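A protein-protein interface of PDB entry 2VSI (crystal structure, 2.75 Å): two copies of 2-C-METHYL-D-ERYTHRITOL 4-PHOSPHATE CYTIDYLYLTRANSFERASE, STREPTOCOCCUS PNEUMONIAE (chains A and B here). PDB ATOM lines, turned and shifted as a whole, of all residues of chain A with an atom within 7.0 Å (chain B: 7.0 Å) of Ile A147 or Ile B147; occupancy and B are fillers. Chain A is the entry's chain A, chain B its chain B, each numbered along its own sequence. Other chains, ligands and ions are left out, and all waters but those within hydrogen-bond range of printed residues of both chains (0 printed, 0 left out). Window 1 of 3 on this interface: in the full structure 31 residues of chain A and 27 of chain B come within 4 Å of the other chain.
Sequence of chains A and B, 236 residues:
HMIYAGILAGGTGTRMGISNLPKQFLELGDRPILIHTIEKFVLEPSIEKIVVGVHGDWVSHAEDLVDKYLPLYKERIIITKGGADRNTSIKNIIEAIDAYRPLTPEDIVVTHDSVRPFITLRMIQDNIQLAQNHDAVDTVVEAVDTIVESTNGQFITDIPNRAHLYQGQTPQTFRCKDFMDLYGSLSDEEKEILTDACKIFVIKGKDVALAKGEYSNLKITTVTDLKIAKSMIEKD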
ATOM      1  N   VAL A 140      -5.014  24.962 -21.497  1.00  0.00           N
ATOM      2  CA  VAL A 140      -3.604  24.831 -21.883  1.00  0.00           C
ATOM      3  C   VAL A 140      -2.788  23.887 -20.995  1.00  0.00           C
ATOM      4  O   VAL A 140      -3.179  23.584 -19.869  1.00  0.00           O
ATOM      5  CB  VAL A 140      -2.893  26.219 -21.908  1.00  0.00           C
ATOM      6  CG1 VAL A 140      -3.439  27.095 -23.038  1.00  0.00           C
ATOM      7  CG2 VAL A 140      -3.000  26.926 -20.544  1.00  0.00           C
ATOM      8  N   ALA A 143       4.444  23.698 -22.166  1.00  0.00           N
ATOM      9  CA  ALA A 143       5.020  23.278 -23.445  1.00  0.00           C
ATOM     10  C   ALA A 143       6.103  22.214 -23.291  1.00  0.00           C
ATOM     11  O   ALA A 143       6.908  22.276 -22.370  1.00  0.00           O
ATOM     12  CB  ALA A 143       5.558  24.490 -24.195  1.00  0.00           C
ATOM     13  N   VAL A 144       6.117  21.238 -24.198  1.00  0.00           N
ATOM     14  CA  VAL A 144       7.074  20.126 -24.112  1.00  0.00           C
ATOM     15  C   VAL A 144       8.241  20.306 -25.085  1.00  0.00           C
ATOM     16  O   VAL A 144       9.403  20.211 -24.682  1.00  0.00           O
ATOM     17  CB  VAL A 144       6.388  18.743 -24.301  1.00  0.00           C
ATOM     18  CG1 VAL A 144       7.386  17.604 -24.102  1.00  0.00           C
ATOM     19  CG2 VAL A 144       5.223  18.594 -23.335  1.00  0.00           C
ATOM     20  N   ASP A 145       7.933  20.568 -26.355  1.00  0.00           N
ATOM     21  CA  ASP A 145       8.972  20.870 -27.347  1.00  0.00           C
ATOM     22  C   ASP A 145       9.611  22.209 -27.045  1.00  0.00           C
ATOM     23  O   ASP A 145       8.992  23.088 -26.433  1.00  0.00           O
ATOM     24  CB  ASP A 145       8.406  20.940 -28.767  1.00  0.00           C
ATOM     25  CG  ASP A 145       7.394  19.867 -29.047  1.00  0.00           C
ATOM     26  OD1 ASP A 145       7.725  18.672 -28.869  1.00  0.00           O
ATOM     27  OD2 ASP A 145       6.267  20.227 -29.459  1.00  0.00           O
ATOM     28  N   THR A 146      10.852  22.357 -27.486  1.00  0.00           N
ATOM     29  CA  THR A 146      11.487  23.661 -27.524  1.00  0.00           C
ATOM     30  C   THR A 146      10.888  24.450 -28.696  1.00  0.00           C
ATOM     31  O   THR A 146      10.849  23.967 -29.827  1.00  0.00           O
ATOM     32  CB  THR A 146      13.038  23.558 -27.590  1.00  0.00           C
ATOM     33  OG1 THR A 146      13.584  24.794 -28.060  1.00  0.00           O
ATOM     34  CG2 THR A 146      13.486  22.427 -28.510  1.00  0.00           C
ATOM     35  N   ILE A 147      10.388  25.646 -28.400  1.00  0.00           N
ATOM     36  CA  ILE A 147       9.727  26.486 -29.400  1.00  0.00           C
ATOM     37  C   ILE A 147      10.675  27.531 -29.997  1.00  0.00           C
ATOM     38  O   ILE A 147      11.380  28.250 -29.274  1.00  0.00           O
ATOM     39  CB  ILE A 147       8.430  27.144 -28.835  1.00  0.00           C
ATOM     40  CG1 ILE A 147       7.278  26.124 -28.759  1.00  0.00           C
ATOM     41  CG2 ILE A 147       8.032  28.392 -29.626  1.00  0.00           C
ATOM     42  CD1 ILE A 147       7.049  25.283 -30.014  1.00  0.00           C
ATOM     43  N   VAL A 148      10.680  27.589 -31.327  1.00  0.00           N
ATOM     44  CA  VAL A 148      11.573  28.451 -32.091  1.00  0.00           C
ATOM     45  C   VAL A 148      10.739  29.398 -32.947  1.00  0.00           C
ATOM     46  O   VAL A 148       9.730  28.992 -33.525  1.00  0.00           O
ATOM     47  CB  VAL A 148      12.548  27.599 -32.955  1.00  0.00           C
ATOM     48  CG1 VAL A 148      13.017  28.355 -34.181  1.00  0.00           C
ATOM     49  CG2 VAL A 148      13.748  27.164 -32.117  1.00  0.00           C
ATOM     50  N   GLU A 149      11.144  30.663 -33.002  1.00  0.00           N
ATOM     51  CA  GLU A 149      10.428  31.640 -33.814  1.00  0.00           C
ATOM     52  C   GLU A 149      11.250  32.069 -35.015  1.00  0.00           C
ATOM     53  O   GLU A 149      12.485  32.080 -34.977  1.00  0.00           O
ATOM     54  CB  GLU A 149      10.012  32.867 -32.999  1.00  0.00           C
ATOM     55  CG  GLU A 149       8.852  33.625 -33.628  1.00  0.00           C
ATOM     56  CD  GLU A 149       8.608  34.968 -32.984  1.00  0.00           C
ATOM     57  OE1 GLU A 149       9.314  35.937 -33.346  1.00  0.00           O
ATOM     58  OE2 GLU A 149       7.699  35.054 -32.128  1.00  0.00           O
ATOM     59  N   ASP A 158      13.731  34.869 -33.083  1.00  0.00           N
ATOM     60  CA  ASP A 158      13.627  34.816 -31.627  1.00  0.00           C
ATOM     61  C   ASP A 158      13.445  33.392 -31.099  1.00  0.00           C
ATOM     62  O   ASP A 158      12.935  32.514 -31.800  1.00  0.00           O
ATOM     63  CB  ASP A 158      12.467  35.695 -31.146  1.00  0.00           C
ATOM     64  CG  ASP A 158      12.478  35.917 -29.643  1.00  0.00           C
ATOM     65  OD1 ASP A 158      13.471  35.551 -28.973  1.00  0.00           O
ATOM     66  OD2 ASP A 158      11.485  36.464 -29.126  1.00  0.00           O
ATOM     67  N   ILE A 159      13.892  33.172 -29.866  1.00  0.00           N
ATOM     68  CA  ILE A 159      13.488  32.007 -29.082  1.00  0.00           C
ATOM     69  C   ILE A 159      12.835  32.522 -27.802  1.00  0.00           C
ATOM     70  O   ILE A 159      13.486  33.203 -27.002  1.00  0.00           O
ATOM     71  CB  ILE A 159      14.666  31.055 -28.752  1.00  0.00           C
ATOM     72  CG1 ILE A 159      15.171  30.371 -30.033  1.00  0.00           C
ATOM     73  CG2 ILE A 159      14.235  30.019 -27.711  1.00  0.00           C
ATOM     74  CD1 ILE A 159      16.285  29.344 -29.837  1.00  0.00           C
ATOM     75  N   PRO A 160      11.534  32.233 -27.620  1.00  0.00           N
ATOM     76  CA  PRO A 160      10.834  32.680 -26.415  1.00  0.00           C
ATOM     77  C   PRO A 160      11.299  31.906 -25.191  1.00  0.00           C
ATOM     78  O   PRO A 160      11.886  30.825 -25.324  1.00  0.00           O
ATOM     79  CB  PRO A 160       9.360  32.368 -26.717  1.00  0.00           C
ATOM     80  CG  PRO A 160       9.302  32.088 -28.196  1.00  0.00           C
ATOM     81  CD  PRO A 160      10.639  31.502 -28.532  1.00  0.00           C
ATOM     82  N   ASN A 161      11.058  32.470 -24.012  1.00  0.00           N
ATOM     83  CA  ASN A 161      11.424  31.817 -22.762  1.00  0.00           C
ATOM     84  C   ASN A 161      10.464  30.669 -22.491  1.00  0.00           C
ATOM     85  O   ASN A 161       9.271  30.879 -22.245  1.00  0.00           O
ATOM     86  CB  ASN A 161      11.448  32.816 -21.603  1.00  0.00           C
ATOM     87  CG  ASN A 161      11.428  32.138 -20.251  1.00  0.00           C
ATOM     88  OD1 ASN A 161      10.555  32.408 -19.431  1.00  0.00           O
ATOM     89  ND2 ASN A 161      12.380  31.238 -20.017  1.00  0.00           N
ATOM     90  N   ARG A 162      11.009  29.457 -22.531  1.00  0.00           N
ATOM     91  CA  ARG A 162      10.210  28.233 -22.559  1.00  0.00           C
ATOM     92  C   ARG A 162       9.487  27.930 -21.249  1.00  0.00           C
ATOM     93  O   ARG A 162       8.727  26.974 -21.171  1.00  0.00           O
ATOM     94  CB  ARG A 162      11.085  27.046 -22.968  1.00  0.00           C
ATOM     95  CG  ARG A 162      10.449  26.161 -24.017  1.00  0.00           C
ATOM     96  CD  ARG A 162      11.034  24.765 -23.987  1.00  0.00           C
ATOM     97  NE  ARG A 162      10.452  23.950 -22.922  1.00  0.00           N
ATOM     98  CZ  ARG A 162      10.840  22.711 -22.627  1.00  0.00           C
ATOM     99  NH1 ARG A 162      11.820  22.138 -23.318  1.00  0.00           N
ATOM    100  NH2 ARG A 162      10.251  22.043 -21.636  1.00  0.00           N
ATOM    101  N   HIS A 164       7.390  29.979 -19.864  1.00  0.00           N
ATOM    102  CA  HIS A 164       6.151  30.745 -19.882  1.00  0.00           C
ATOM    103  C   HIS A 164       5.310  30.356 -21.083  1.00  0.00           C
ATOM    104  O   HIS A 164       4.257  30.945 -21.335  1.00  0.00           O
ATOM    105  CB  HIS A 164       6.438  32.254 -19.893  1.00  0.00           C
ATOM    106  CG  HIS A 164       6.916  32.788 -18.578  1.00  0.00           C
ATOM    107  ND1 HIS A 164       8.124  33.434 -18.433  1.00  0.00           N
ATOM    108  CD2 HIS A 164       6.350  32.770 -17.347  1.00  0.00           C
ATOM    109  CE1 HIS A 164       8.281  33.794 -17.171  1.00  0.00           C
ATOM    110  NE2 HIS A 164       7.219  33.402 -16.492  1.00  0.00           N
ATOM    111  N   LEU A 165       5.786  29.359 -21.819  1.00  0.00           N
ATOM    112  CA  LEU A 165       5.081  28.853 -22.987  1.00  0.00           C
ATOM    113  C   LEU A 165       4.183  27.689 -22.632  1.00  0.00           C
ATOM    114  O   LEU A 165       4.549  26.803 -21.859  1.00  0.00           O
ATOM    115  CB  LEU A 165       6.057  28.431 -24.080  1.00  0.00           C
ATOM    116  CG  LEU A 165       6.979  29.519 -24.615  1.00  0.00           C
ATOM    117  CD1 LEU A 165       7.908  28.920 -25.647  1.00  0.00           C
ATOM    118  CD2 LEU A 165       6.173  30.676 -25.192  1.00  0.00           C
ATOM    119  N   TYR A 166       2.999  27.711 -23.221  1.00  0.00           N
ATOM    120  CA  TYR A 166       1.992  26.701 -22.990  1.00  0.00           C
ATOM    121  C   TYR A 166       1.537  26.150 -24.322  1.00  0.00           C
ATOM    122  O   TYR A 166       1.420  26.882 -25.309  1.00  0.00           O
ATOM    123  CB  TYR A 166       0.802  27.308 -22.241  1.00  0.00           C
ATOM    124  CG  TYR A 166       1.144  27.756 -20.846  1.00  0.00           C
ATOM    125  CD1 TYR A 166       1.654  29.028 -20.605  1.00  0.00           C
ATOM    126  CD2 TYR A 166       0.978  26.899 -19.765  1.00  0.00           C
ATOM    127  CE1 TYR A 166       1.987  29.441 -19.310  1.00  0.00           C
ATOM    128  CE2 TYR A 166       1.307  27.301 -18.471  1.00  0.00           C
ATOM    129  CZ  TYR A 166       1.807  28.569 -18.256  1.00  0.00           C
ATOM    130  OH  TYR A 166       2.123  28.955 -16.984  1.00  0.00           O
ATOM    131  N   GLN A 167       1.304  24.847 -24.353  1.00  0.00           N
ATOM    132  CA  GLN A 167       0.679  24.225 -25.497  1.00  0.00           C
ATOM    133  C   GLN A 167      -0.823  24.422 -25.364  1.00  0.00           C
ATOM    134  O   GLN A 167      -1.435  24.002 -24.377  1.00  0.00           O
ATOM    135  CB  GLN A 167       1.032  22.744 -25.550  1.00  0.00           C
ATOM    136  CG  GLN A 167       0.420  21.999 -26.712  1.00  0.00           C
ATOM    137  CD  GLN A 167       0.377  20.516 -26.454  1.00  0.00           C
ATOM    138  OE1 GLN A 167      -0.427  20.040 -25.642  1.00  0.00           O
ATOM    139  NE2 GLN A 167       1.247  19.769 -27.134  1.00  0.00           N
ATOM    140  N   GLY A 168      -1.402  25.084 -26.359  1.00  0.00           N
ATOM    141  CA  GLY A 168      -2.808  25.438 -26.336  1.00  0.00           C
ATOM    142  C   GLY A 168      -3.681  24.322 -26.849  1.00  0.00           C
ATOM    143  O   GLY A 168      -3.435  23.772 -27.914  1.00  0.00           O
ATOM    144  N   ALA B 143       5.227  24.559 -36.106  1.00  0.00           N
ATOM    145  CA  ALA B 143       4.430  24.214 -34.934  1.00  0.00           C
ATOM    146  C   ALA B 143       3.049  23.779 -35.393  1.00  0.00           C
ATOM    147  O   ALA B 143       2.448  24.437 -36.248  1.00  0.00           O
ATOM    148  CB  ALA B 143       4.323  25.401 -33.997  1.00  0.00           C
ATOM    149  N   VAL B 144       2.569  22.658 -34.858  1.00  0.00           N
ATOM    150  CA  VAL B 144       1.198  22.221 -35.111  1.00  0.00           C
ATOM    151  C   VAL B 144       0.257  22.722 -34.028  1.00  0.00           C
ATOM    152  O   VAL B 144      -0.942  22.850 -34.260  1.00  0.00           O
ATOM    153  CB  VAL B 144       1.068  20.697 -35.214  1.00  0.00           C
ATOM    154  CG1 VAL B 144       1.731  20.196 -36.493  1.00  0.00           C
ATOM    155  CG2 VAL B 144       1.639  20.009 -33.971  1.00  0.00           C
ATOM    156  N   ASP B 145       0.810  22.998 -32.849  1.00  0.00           N
ATOM    157  CA  ASP B 145       0.030  23.474 -31.713  1.00  0.00           C
ATOM    158  C   ASP B 145       0.077  24.991 -31.647  1.00  0.00           C
ATOM    159  O   ASP B 145       1.122  25.602 -31.910  1.00  0.00           O
ATOM    160  CB  ASP B 145       0.572  22.912 -30.387  1.00  0.00           C
ATOM    161  CG  ASP B 145       0.585  21.379 -30.332  1.00  0.00           C
ATOM    162  OD1 ASP B 145      -0.335  20.732 -30.885  1.00  0.00           O
ATOM    163  OD2 ASP B 145       1.522  20.828 -29.708  1.00  0.00           O
ATOM    164  N   THR B 146      -1.058  25.592 -31.291  1.00  0.00           N
ATOM    165  CA  THR B 146      -1.108  26.996 -30.911  1.00  0.00           C
ATOM    166  C   THR B 146      -0.270  27.135 -29.646  1.00  0.00           C
ATOM    167  O   THR B 146      -0.495  26.422 -28.664  1.00  0.00           O
ATOM    168  CB  THR B 146      -2.562  27.453 -30.658  1.00  0.00           C
ATOM    169  OG1 THR B 146      -3.247  27.573 -31.908  1.00  0.00           O
ATOM    170  CG2 THR B 146      -2.619  28.795 -29.934  1.00  0.00           C
ATOM    171  N   ILE B 147       0.723  28.016 -29.685  1.00  0.00           N
ATOM    172  CA  ILE B 147       1.541  28.279 -28.507  1.00  0.00           C
ATOM    173  C   ILE B 147       1.009  29.510 -27.789  1.00  0.00           C
ATOM    174  O   ILE B 147       0.769  30.544 -28.408  1.00  0.00           O
ATOM    175  CB  ILE B 147       3.052  28.426 -28.848  1.00  0.00           C
ATOM    176  CG1 ILE B 147       3.593  27.164 -29.543  1.00  0.00           C
ATOM    177  CG2 ILE B 147       3.870  28.746 -27.600  1.00  0.00           C
ATOM    178  CD1 ILE B 147       3.318  25.837 -28.825  1.00  0.00           C
ATOM    179  N   VAL B 148       0.813  29.375 -26.482  1.00  0.00           N
ATOM    180  CA  VAL B 148       0.216  30.418 -25.663  1.00  0.00           C
ATOM    181  C   VAL B 148       1.225  30.882 -24.626  1.00  0.00           C
ATOM    182  O   VAL B 148       1.771  30.075 -23.872  1.00  0.00           O
ATOM    183  CB  VAL B 148      -1.062  29.909 -24.946  1.00  0.00           C
ATOM    184  CG1 VAL B 148      -1.661  30.988 -24.061  1.00  0.00           C
ATOM    185  CG2 VAL B 148      -2.095  29.413 -25.960  1.00  0.00           C
ATOM    186  N   GLU B 149       1.471  32.184 -24.589  1.00  0.00           N
ATOM    187  CA  GLU B 149       2.373  32.742 -23.604  1.00  0.00           C
ATOM    188  C   GLU B 149       1.603  33.352 -22.434  1.00  0.00           C
ATOM    189  O   GLU B 149       0.586  34.020 -22.625  1.00  0.00           O
ATOM    190  CB  GLU B 149       3.288  33.779 -24.256  1.00  0.00           C
ATOM    191  CG  GLU B 149       4.588  34.023 -23.504  1.00  0.00           C
ATOM    192  CD  GLU B 149       5.368  35.197 -24.056  1.00  0.00           C
ATOM    193  OE1 GLU B 149       6.412  34.955 -24.707  1.00  0.00           O
ATOM    194  OE2 GLU B 149       4.933  36.354 -23.843  1.00  0.00           O
ATOM    195  N   ASP B 158       0.106  36.765 -24.198  1.00  0.00           N
ATOM    196  CA  ASP B 158       0.472  36.689 -25.617  1.00  0.00           C
ATOM    197  C   ASP B 158       0.117  35.360 -26.313  1.00  0.00           C
ATOM    198  O   ASP B 158       0.381  34.277 -25.787  1.00  0.00           O
ATOM    199  CB  ASP B 158       1.978  36.955 -25.771  1.00  0.00           C
ATOM    200  CG  ASP B 158       2.391  37.245 -27.204  1.00  0.00           C
ATOM    201  OD1 ASP B 158       1.538  37.194 -28.115  1.00  0.00           O
ATOM    202  OD2 ASP B 158       3.586  37.524 -27.417  1.00  0.00           O
ATOM    203  N   ILE B 159      -0.471  35.459 -27.502  1.00  0.00           N
ATOM    204  CA  ILE B 159      -0.560  34.315 -28.412  1.00  0.00           C
ATOM    205  C   ILE B 159       0.181  34.666 -29.703  1.00  0.00           C
ATOM    206  O   ILE B 159      -0.381  35.317 -30.588  1.00  0.00           O
ATOM    207  CB  ILE B 159      -2.020  33.868 -28.724  1.00  0.00           C
ATOM    208  CG1 ILE B 159      -2.784  33.550 -27.434  1.00  0.00           C
ATOM    209  CG2 ILE B 159      -2.011  32.637 -29.654  1.00  0.00           C
ATOM    210  CD1 ILE B 159      -4.237  33.223 -27.635  1.00  0.00           C
ATOM    211  N   PRO B 160       1.450  34.243 -29.817  1.00  0.00           N
ATOM    212  CA  PRO B 160       2.234  34.602 -30.985  1.00  0.00           C
ATOM    213  C   PRO B 160       1.550  34.126 -32.247  1.00  0.00           C
ATOM    214  O   PRO B 160       0.677  33.269 -32.180  1.00  0.00           O
ATOM    215  CB  PRO B 160       3.532  33.824 -30.784  1.00  0.00           C
ATOM    216  CG  PRO B 160       3.629  33.634 -29.318  1.00  0.00           C
ATOM    217  CD  PRO B 160       2.220  33.408 -28.880  1.00  0.00           C
ATOM    218  N   ASN B 161       1.925  34.696 -33.385  1.00  0.00           N
ATOM    219  CA  ASN B 161       1.488  34.172 -34.672  1.00  0.00           C
ATOM    220  C   ASN B 161       2.063  32.775 -34.850  1.00  0.00           C
ATOM    221  O   ASN B 161       3.273  32.570 -34.711  1.00  0.00           O
ATOM    222  CB  ASN B 161       1.943  35.083 -35.811  1.00  0.00           C
ATOM    223  CG  ASN B 161       1.318  34.716 -37.133  1.00  0.00           C
ATOM    224  OD1 ASN B 161       0.810  33.609 -37.316  1.00  0.00           O
ATOM    225  ND2 ASN B 161       1.355  35.646 -38.071  1.00  0.00           N
ATOM    226  N   ARG B 162       1.190  31.816 -35.129  1.00  0.00           N
ATOM    227  CA  ARG B 162       1.606  30.423 -35.258  1.00  0.00           C
ATOM    228  C   ARG B 162       2.388  30.180 -36.541  1.00  0.00           C
ATOM    229  O   ARG B 162       3.246  29.297 -36.601  1.00  0.00           O
ATOM    230  CB  ARG B 162       0.395  29.495 -35.199  1.00  0.00           C
ATOM    231  CG  ARG B 162       0.760  28.045 -34.960  1.00  0.00           C
ATOM    232  CD  ARG B 162      -0.435  27.231 -34.498  1.00  0.00           C
ATOM    233  NE  ARG B 162      -1.385  26.968 -35.573  1.00  0.00           N
ATOM    234  CZ  ARG B 162      -1.153  26.144 -36.590  1.00  0.00           C
ATOM    235  NH1 ARG B 162       0.006  25.503 -36.683  1.00  0.00           N
ATOM    236  NH2 ARG B 162      -2.081  25.964 -37.520  1.00  0.00           N
ATOM    237  N   LEU B 165       6.100  30.210 -35.981  1.00  0.00           N
ATOM    238  CA  LEU B 165       6.607  29.405 -34.880  1.00  0.00           C
ATOM    239  C   LEU B 165       6.996  28.005 -35.306  1.00  0.00           C
ATOM    240  O   LEU B 165       6.364  27.413 -36.187  1.00  0.00           O
ATOM    241  CB  LEU B 165       5.582  29.349 -33.744  1.00  0.00           C
ATOM    242  CG  LEU B 165       5.470  30.567 -32.826  1.00  0.00           C
ATOM    243  CD1 LEU B 165       4.383  30.345 -31.786  1.00  0.00           C
ATOM    244  CD2 LEU B 165       6.798  30.869 -32.146  1.00  0.00           C
ATOM    245  N   TYR B 166       8.027  27.471 -34.653  1.00  0.00           N
ATOM    246  CA  TYR B 166       8.616  26.194 -35.049  1.00  0.00           C
ATOM    247  C   TYR B 166       8.939  25.256 -33.890  1.00  0.00           C
ATOM    248  O   TYR B 166       9.328  25.694 -32.807  1.00  0.00           O
ATOM    249  CB  TYR B 166       9.856  26.444 -35.910  1.00  0.00           C
ATOM    250  CG  TYR B 166       9.499  27.142 -37.196  1.00  0.00           C
ATOM    251  CD1 TYR B 166       8.962  26.429 -38.262  1.00  0.00           C
ATOM    252  CD2 TYR B 166       9.646  28.523 -37.330  1.00  0.00           C
ATOM    253  CE1 TYR B 166       8.609  27.056 -39.436  1.00  0.00           C
ATOM    254  CE2 TYR B 166       9.290  29.164 -38.504  1.00  0.00           C
ATOM    255  CZ  TYR B 166       8.773  28.421 -39.556  1.00  0.00           C
ATOM    256  OH  TYR B 166       8.415  29.040 -40.736  1.00  0.00           O
ATOM    257  N   GLN B 167       8.760  23.961 -34.124  1.00  0.00           N
ATOM    258  CA  GLN B 167       9.173  22.955 -33.161  1.00  0.00           C
ATOM    259  C   GLN B 167      10.631  22.614 -33.386  1.00  0.00           C
ATOM    260  O   GLN B 167      11.040  22.318 -34.510  1.00  0.00           O
ATOM    261  CB  GLN B 167       8.324  21.692 -33.279  1.00  0.00           C
ATOM    262  CG  GLN B 167       6.921  21.841 -32.707  1.00  0.00           C
ATOM    263  CD  GLN B 167       6.035  20.637 -32.982  1.00  0.00           C
ATOM    264  OE1 GLN B 167       4.812  20.772 -33.078  1.00  0.00           O
ATOM    265  NE2 GLN B 167       6.646  19.455 -33.112  1.00  0.00           N
ATOM    266  N   GLY B 168      11.407  22.664 -32.309  1.00  0.00           N
ATOM    267  CA  GLY B 168      12.812  22.298 -32.350  1.00  0.00           C
ATOM    268  C   GLY B 168      12.970  20.803 -32.505  1.00  0.00           C
ATOM    269  O   GLY B 168      12.234  20.028 -31.899  1.00  0.00           O
ATOM    270  N   LYS B 199      20.143  27.900 -28.612  1.00  0.00           N
ATOM    271  CA  LYS B 199      19.750  29.019 -27.760  1.00  0.00           C
ATOM    272  C   LYS B 199      20.966  29.864 -27.363  1.00  0.00           C
ATOM    273  O   LYS B 199      20.831  31.054 -27.076  1.00  0.00           O
ATOM    274  CB  LYS B 199      19.007  28.513 -26.518  1.00  0.00           C
ATOM    275  CG  LYS B 199      18.099  29.542 -25.850  1.00  0.00           C
ATOM    276  CD  LYS B 199      17.279  28.909 -24.728  1.00  0.00           C
ATOM    277  CE  LYS B 199      16.558  29.956 -23.886  1.00  0.00           C
ATOM    278  NZ  LYS B 199      15.412  30.586 -24.599  1.00  0.00           N
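O of Asp A158 sits at hydrogen-bond distance from N of Glu A149 (2.8 Å). The backbone NH (N) of Val B144 sits close to the side-chain amide oxygen (OE1) of Gln B167, 3.4 Å away. N of Ala B143 sits at hydrogen-bond distance from O of Leu B165, 3.1 Å away. The side-chain amide oxygen (OD1) of Asn A161 sits at hydrogen-bond distance from a ring nitrogen (ND1) of His A164, at 2.8 Å. N of Ala A143 sits at hydrogen-bond distance from O of Leu A165, 3.1 Å away. The backbone NH (N) of Glu B149 lies within hydrogen-bond range of the backbone carbonyl oxygen (O) of Asp B158 (2.6 Å).
The side-chain amide nitrogen of Gln A167 is in hydrogen-bond range of the side-chain carboxylate of Asp B145 (2.8 Å). The backbone NH (N) of Tyr A166 sits at hydrogen-bond distance from the backbone carbonyl oxygen (O) of Val B148, 2.7 Å away. N of Tyr B166 lies within hydrogen-bond range of O of Val A148. O of Thr B146 lies within hydrogen-bond range of N of Gly A168 (2.8 Å). The backbone NH (N) of Gly B168 sits at hydrogen-bond distance from the backbone carbonyl oxygen (O) of Thr A146 (2.9 Å).
CG2 of Val B148 touches CG1 of Val A140, 3.96 Å away. O of Thr A146 touches O of Tyr B166, at 3.8 Å. CD2 of Leu B165 touches CG2 of Ile A147 (3.7 Å). O of Tyr B166 touches CA of Ile A147, at 3.5 Å. CG of Glu A149 touches CD2 of Leu B165, 3.7 Å away. Pro A160 touches Lys B199 (O to NZ, 3.6 Å). O of His A164 touches O of Val B148 (3.7 Å). O of His A164 touches CA of Glu B149, at 3.5 Å. Val B148 touches Leu A165 (O to C, 3.6 Å). Gln A167 touches Thr B146.
Ile A147 touches its own counterpart, Ile B147. Ile A147 touches Leu B165, and with the chains exchanged Leu A165 touches Ile B147. Ile A147 touches Tyr B166, and with the chains exchanged Tyr A166 touches Ile B147. Val A148 touches Tyr B166, and with the chains exchanged Tyr A166 touches Val B148. Positions printed for both chains: 143, 144, 145, 146, 147, 148, 149, 158, 159, 160, 161, 162, 165, 166, 167 and 168.
Of chain B, only Ile B147, Leu B165 and Tyr B166 come within 4 Å of Ile A147. Of chain A, only Ile A147 (3.9 Å), Leu A165 (3.9 Å) and Tyr A166 (3.5 Å) come within 4 Å of Ile B147. Of the printed residues of chain B, Pro A160 touches Lys B199 (3.6 Å). Printed residues of chain A within 4 Å of Gly B168: Thr A146. Of the printed residues of chain A, Leu B165 touches Ile A147, Val A148 and Glu A149. Asp A158 touches none of the printed residues of chain B. Val B144 touches none of the printed residues of chain A. The nearest residue of chain B that does not touch Ile A147 is Gln B167 (4.4 Å). The nearest residue of chain A that does not touch Ile B147 is Gln A167 (4.5 Å). The nearest printed residue of chain A that does not touch Gln B167 is Ile A147 (4.4 Å).
Printed residues of chain A that touch a printed residue of chain B: Val A140, Asp A145, Thr A146, Ile A147, Val A148, Glu A149, Ile A159, Pro A160, His A164, Leu A165, Tyr A166, Gln A167 and Gly A168. Hydrophobic or aromatic side chains of chain A within 4 Å of the printed part of chain B: Val A140, Ile A147, Val A148, Ile A159, Leu A165 and Tyr A166. Printed residues of chain B that touch a printed residue of chain A: Asp B145, Thr B146, Ile B147, Val B148, Glu B149, Leu B165, Tyr B166, Gln B167, Gly B168 and Lys B199. Hydrophobic or aromatic side chains of chain B within 4 Å of the printed part of chain A: Ile B147, Val B148, Leu B165 and Tyr B166. Among the printed residues, no Asp or Glu carboxylate lies within 4 Å of a Lys or Arg side-chain nitrogen of the other chain.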
